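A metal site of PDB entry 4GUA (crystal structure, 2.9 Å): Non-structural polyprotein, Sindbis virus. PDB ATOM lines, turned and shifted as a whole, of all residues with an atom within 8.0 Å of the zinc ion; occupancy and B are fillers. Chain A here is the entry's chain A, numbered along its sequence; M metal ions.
OG of Ser 631 sits at hydrogen-bond distance from N of Cys 648 (3.3 Å). A ring nitrogen (NE2) of His 522 lies within hydrogen-bond range of the backbone carbonyl oxygen (O) of Cys 607 (2.9 Å). The side-chain sulfur (SG) of Cys 648 lies close to the backbone carbonyl oxygen (O) of Lys 650. The backbone NH (N) of Tyr 609 lies close to the side-chain sulfur (SG) of Cys 607 (3.2 Å). The side-chain sulfur of Cys 630 lies close to the backbone NH of Ser 632. The side-chain sulfur (SG) of Cys 648 lies close to the side-chain hydroxyl (OG) of Ser 632 (3.5 Å).
Four residues have an atom within 4 Å of the zinc ion: Cys 605, Cys 607, Cys 630 and Cys 648.
The zinc ion is bound by SG of Cys 630, SG of Cys 648, SG of Cys 605 and SG of Cys 607. The zinc ion has four donor atoms within binding distance.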
ATOM      1  N   HIS A 522       6.214  21.491  10.035  1.00  0.00           N
ATOM      2  CA  HIS A 522       7.378  21.679  10.892  1.00  0.00           C
ATOM      3  C   HIS A 522       7.551  23.173  11.243  1.00  0.00           C
ATOM      4  O   HIS A 522       7.317  24.037  10.402  1.00  0.00           O
ATOM      5  CB  HIS A 522       8.617  21.149  10.175  1.00  0.00           C
ATOM      6  CG  HIS A 522       9.831  21.062  11.041  1.00  0.00           C
ATOM      7  ND1 HIS A 522      10.814  22.019  11.044  1.00  0.00           N
ATOM      8  CD2 HIS A 522      10.214  20.127  11.946  1.00  0.00           C
ATOM      9  CE1 HIS A 522      11.758  21.680  11.907  1.00  0.00           C
ATOM     10  NE2 HIS A 522      11.414  20.536  12.467  1.00  0.00           N
ATOM     11  N   PRO A 604       7.661  14.201  10.642  1.00  0.00           N
ATOM     12  CA  PRO A 604       8.357  12.987  11.101  1.00  0.00           C
ATOM     13  C   PRO A 604       9.118  13.207  12.400  1.00  0.00           C
ATOM     14  O   PRO A 604       9.273  12.286  13.214  1.00  0.00           O
ATOM     15  CB  PRO A 604       9.304  12.667   9.952  1.00  0.00           C
ATOM     16  CG  PRO A 604       9.498  13.970   9.239  1.00  0.00           C
ATOM     17  CD  PRO A 604       8.207  14.699   9.367  1.00  0.00           C
ATOM     18  N   CYS A 605       9.607  14.432  12.592  1.00  0.00           N
ATOM     19  CA  CYS A 605      10.182  14.822  13.873  1.00  0.00           C
ATOM     20  C   CYS A 605      10.213  16.338  13.970  1.00  0.00           C
ATOM     21  O   CYS A 605       9.879  17.028  13.008  1.00  0.00           O
ATOM     22  CB  CYS A 605      11.574  14.241  14.063  1.00  0.00           C
ATOM     23  SG  CYS A 605      12.819  14.840  12.907  1.00  0.00           S
ATOM     24  N   LEU A 606      10.607  16.840  15.138  1.00  0.00           N
ATOM     25  CA  LEU A 606      10.668  18.279  15.363  1.00  0.00           C
ATOM     26  C   LEU A 606      12.069  18.878  15.241  1.00  0.00           C
ATOM     27  O   LEU A 606      12.240  20.093  15.357  1.00  0.00           O
ATOM     28  CB  LEU A 606      10.087  18.613  16.735  1.00  0.00           C
ATOM     29  CG  LEU A 606       8.631  18.179  16.872  1.00  0.00           C
ATOM     30  CD1 LEU A 606       8.085  18.567  18.234  1.00  0.00           C
ATOM     31  CD2 LEU A 606       7.800  18.786  15.751  1.00  0.00           C
ATOM     32  N   CYS A 607      13.066  18.039  14.973  1.00  0.00           N
ATOM     33  CA  CYS A 607      14.445  18.506  14.933  1.00  0.00           C
ATOM     34  C   CYS A 607      14.743  19.118  13.557  1.00  0.00           C
ATOM     35  O   CYS A 607      13.899  19.082  12.659  1.00  0.00           O
ATOM     36  CB  CYS A 607      15.430  17.367  15.246  1.00  0.00           C
ATOM     37  SG  CYS A 607      16.050  16.451  13.808  1.00  0.00           S
ATOM     38  N   MET A 608      15.944  19.667  13.411  1.00  0.00           N
ATOM     39  CA  MET A 608      16.290  20.435  12.203  1.00  0.00           C
ATOM     40  C   MET A 608      16.482  19.554  10.974  1.00  0.00           C
ATOM     41  O   MET A 608      16.556  20.058   9.856  1.00  0.00           O
ATOM     42  CB  MET A 608      17.563  21.253  12.427  1.00  0.00           C
ATOM     43  CG  MET A 608      18.838  20.424  12.479  1.00  0.00           C
ATOM     44  SD  MET A 608      20.260  21.383  13.034  1.00  0.00           S
ATOM     45  CE  MET A 608      20.344  22.641  11.762  1.00  0.00           C
ATOM     46  N   TYR A 609      16.607  18.243  11.199  1.00  0.00           N
ATOM     47  CA  TYR A 609      16.859  17.306  10.102  1.00  0.00           C
ATOM     48  C   TYR A 609      15.598  16.604   9.597  1.00  0.00           C
ATOM     49  O   TYR A 609      15.658  15.799   8.675  1.00  0.00           O
ATOM     50  CB  TYR A 609      17.918  16.291  10.542  1.00  0.00           C
ATOM     51  CG  TYR A 609      19.213  16.948  10.950  1.00  0.00           C
ATOM     52  CD1 TYR A 609      20.016  17.599  10.011  1.00  0.00           C
ATOM     53  CD2 TYR A 609      19.632  16.947  12.267  1.00  0.00           C
ATOM     54  CE1 TYR A 609      21.193  18.210  10.374  1.00  0.00           C
ATOM     55  CE2 TYR A 609      20.820  17.567  12.654  1.00  0.00           C
ATOM     56  CZ  TYR A 609      21.595  18.194  11.695  1.00  0.00           C
ATOM     57  OH  TYR A 609      22.775  18.813  12.046  1.00  0.00           O
ATOM     58  N   ALA A 610      14.448  16.951  10.177  1.00  0.00           N
ATOM     59  CA  ALA A 610      13.204  16.254   9.874  1.00  0.00           C
ATOM     60  C   ALA A 610      13.011  16.153   8.372  1.00  0.00           C
ATOM     61  O   ALA A 610      13.151  17.142   7.672  1.00  0.00           O
ATOM     62  CB  ALA A 610      12.035  16.998  10.477  1.00  0.00           C
ATOM     63  N   MET A 611      12.678  14.964   7.863  1.00  0.00           N
ATOM     64  CA  MET A 611      12.686  14.808   6.421  1.00  0.00           C
ATOM     65  C   MET A 611      11.270  15.017   5.918  1.00  0.00           C
ATOM     66  O   MET A 611      10.477  14.099   5.785  1.00  0.00           O
ATOM     67  CB  MET A 611      13.147  13.387   6.099  1.00  0.00           C
ATOM     68  CG  MET A 611      13.664  13.182   4.685  1.00  0.00           C
ATOM     69  SD  MET A 611      15.340  13.806   4.442  1.00  0.00           S
ATOM     70  CE  MET A 611      16.266  12.815   5.597  1.00  0.00           C
ATOM     71  N   ARG A 615      12.304  19.717   3.193  1.00  0.00           N
ATOM     72  CA  ARG A 615      13.739  19.526   3.381  1.00  0.00           C
ATOM     73  C   ARG A 615      14.349  18.786   2.211  1.00  0.00           C
ATOM     74  O   ARG A 615      15.445  19.103   1.771  1.00  0.00           O
ATOM     75  CB  ARG A 615      14.042  18.774   4.671  1.00  0.00           C
ATOM     76  CG  ARG A 615      15.541  18.592   4.870  1.00  0.00           C
ATOM     77  CD  ARG A 615      15.923  18.421   6.327  1.00  0.00           C
ATOM     78  NE  ARG A 615      17.357  18.155   6.485  1.00  0.00           N
ATOM     79  CZ  ARG A 615      17.906  16.948   6.544  1.00  0.00           C
ATOM     80  NH1 ARG A 615      17.169  15.844   6.469  1.00  0.00           N
ATOM     81  NH2 ARG A 615      19.219  16.843   6.684  1.00  0.00           N
ATOM     82  N   VAL A 629      21.072  12.676   8.420  1.00  0.00           N
ATOM     83  CA  VAL A 629      19.779  12.072   8.707  1.00  0.00           C
ATOM     84  C   VAL A 629      19.672  11.737  10.177  1.00  0.00           C
ATOM     85  O   VAL A 629      20.611  11.208  10.777  1.00  0.00           O
ATOM     86  CB  VAL A 629      19.591  10.781   7.895  1.00  0.00           C
ATOM     87  CG1 VAL A 629      18.280  10.108   8.253  1.00  0.00           C
ATOM     88  CG2 VAL A 629      19.662  11.089   6.408  1.00  0.00           C
ATOM     89  N   CYS A 630      18.528  12.044  10.785  1.00  0.00           N
ATOM     90  CA  CYS A 630      18.342  11.766  12.198  1.00  0.00           C
ATOM     91  C   CYS A 630      17.728  10.393  12.430  1.00  0.00           C
ATOM     92  O   CYS A 630      17.362   9.700  11.478  1.00  0.00           O
ATOM     93  CB  CYS A 630      17.477  12.841  12.852  1.00  0.00           C
ATOM     94  SG  CYS A 630      15.780  12.867  12.268  1.00  0.00           S
ATOM     95  N   SER A 631      17.580  10.009  13.692  1.00  0.00           N
ATOM     96  CA  SER A 631      17.143   8.665  14.039  1.00  0.00           C
ATOM     97  C   SER A 631      15.647   8.471  13.784  1.00  0.00           C
ATOM     98  O   SER A 631      15.159   7.333  13.757  1.00  0.00           O
ATOM     99  CB  SER A 631      17.462   8.365  15.512  1.00  0.00           C
ATOM    100  OG  SER A 631      16.652   9.127  16.390  1.00  0.00           O
ATOM    101  N   SER A 632      14.927   9.570  13.587  1.00  0.00           N
ATOM    102  CA  SER A 632      13.497   9.498  13.252  1.00  0.00           C
ATOM    103  C   SER A 632      13.298   9.247  11.765  1.00  0.00           C
ATOM    104  O   SER A 632      12.173   9.170  11.282  1.00  0.00           O
ATOM    105  CB  SER A 632      12.765  10.767  13.675  1.00  0.00           C
ATOM    106  OG  SER A 632      12.640  10.832  15.087  1.00  0.00           O
ATOM    107  N   THR A 633      14.397   9.129  11.038  1.00  0.00           N
ATOM    108  CA  THR A 633      14.334   8.659   9.664  1.00  0.00           C
ATOM    109  C   THR A 633      15.162   7.386   9.614  1.00  0.00           C
ATOM    110  O   THR A 633      16.348   7.414   9.285  1.00  0.00           O
ATOM    111  CB  THR A 633      14.883   9.698   8.693  1.00  0.00           C
ATOM    112  OG1 THR A 633      14.021  10.835   8.675  1.00  0.00           O
ATOM    113  CG2 THR A 633      14.999   9.134   7.290  1.00  0.00           C
ATOM    114  N   VAL A 646      22.752  10.684  12.645  1.00  0.00           N
ATOM    115  CA  VAL A 646      22.802  11.372  13.932  1.00  0.00           C
ATOM    116  C   VAL A 646      21.495  11.151  14.683  1.00  0.00           C
ATOM    117  O   VAL A 646      20.494  10.746  14.089  1.00  0.00           O
ATOM    118  CB  VAL A 646      23.035  12.882  13.763  1.00  0.00           C
ATOM    119  CG1 VAL A 646      24.255  13.133  12.902  1.00  0.00           C
ATOM    120  CG2 VAL A 646      21.811  13.562  13.172  1.00  0.00           C
ATOM    121  N   GLN A 647      21.499  11.433  15.978  1.00  0.00           N
ATOM    122  CA  GLN A 647      20.330  11.225  16.809  1.00  0.00           C
ATOM    123  C   GLN A 647      19.339  12.378  16.664  1.00  0.00           C
ATOM    124  O   GLN A 647      19.750  13.528  16.478  1.00  0.00           O
ATOM    125  CB  GLN A 647      20.740  11.043  18.266  1.00  0.00           C
ATOM    126  CG  GLN A 647      21.101  12.324  18.990  1.00  0.00           C
ATOM    127  CD  GLN A 647      21.873  12.074  20.270  1.00  0.00           C
ATOM    128  OE1 GLN A 647      22.718  11.171  20.328  1.00  0.00           O
ATOM    129  NE2 GLN A 647      21.600  12.865  21.298  1.00  0.00           N
ATOM    130  N   CYS A 648      18.051  12.062  16.750  1.00  0.00           N
ATOM    131  CA  CYS A 648      17.011  13.087  16.752  1.00  0.00           C
ATOM    132  C   CYS A 648      16.789  13.595  18.165  1.00  0.00           C
ATOM    133  O   CYS A 648      16.513  12.818  19.087  1.00  0.00           O
ATOM    134  CB  CYS A 648      15.707  12.529  16.184  1.00  0.00           C
ATOM    135  SG  CYS A 648      14.376  13.758  16.089  1.00  0.00           S
ATOM    136  N   THR A 649      16.943  14.905  18.337  1.00  0.00           N
ATOM    137  CA  THR A 649      16.861  15.536  19.654  1.00  0.00           C
ATOM    138  C   THR A 649      15.441  15.891  20.131  1.00  0.00           C
ATOM    139  O   THR A 649      15.226  16.088  21.325  1.00  0.00           O
ATOM    140  CB  THR A 649      17.718  16.800  19.686  1.00  0.00           C
ATOM    141  OG1 THR A 649      17.224  17.736  18.715  1.00  0.00           O
ATOM    142  CG2 THR A 649      19.166  16.461  19.352  1.00  0.00           C
ATOM    143  N   LYS A 650      14.499  15.993  19.196  1.00  0.00           N
ATOM    144  CA  LYS A 650      13.089  16.194  19.544  1.00  0.00           C
ATOM    145  C   LYS A 650      12.176  15.367  18.630  1.00  0.00           C
ATOM    146  O   LYS A 650      12.213  15.524  17.406  1.00  0.00           O
ATOM    147  CB  LYS A 650      12.720  17.683  19.437  1.00  0.00           C
ATOM    148  N   VAL A 651      11.346  14.511  19.214  1.00  0.00           N
ATOM    149  CA  VAL A 651      10.598  13.541  18.406  1.00  0.00           C
ATOM    150  C   VAL A 651       9.083  13.714  18.470  1.00  0.00           C
ATOM    151  O   VAL A 651       8.570  14.544  19.233  1.00  0.00           O
ATOM    152  CB  VAL A 651      10.930  12.088  18.833  1.00  0.00           C
ATOM    153  CG1 VAL A 651      12.377  11.767  18.511  1.00  0.00           C
ATOM    154  CG2 VAL A 651      10.622  11.864  20.305  1.00  0.00           C
ATOM    155  N   VAL A 652       8.391  12.920  17.665  1.00  0.00           N
ATOM    156  CA  VAL A 652       6.925  12.866  17.681  1.00  0.00           C
ATOM    157  C   VAL A 652       6.478  11.458  18.054  1.00  0.00           C
ATOM    158  O   VAL A 652       7.160  10.484  17.762  1.00  0.00           O
ATOM    159  CB  VAL A 652       6.305  13.271  16.328  1.00  0.00           C
ATOM    160  CG1 VAL A 652       6.682  14.699  15.995  1.00  0.00           C
ATOM    161  CG2 VAL A 652       6.752  12.330  15.227  1.00  0.00           C
HETATM  162 ZN    ZN M   1      14.897  14.212  13.875  1.00  0.00          ZN
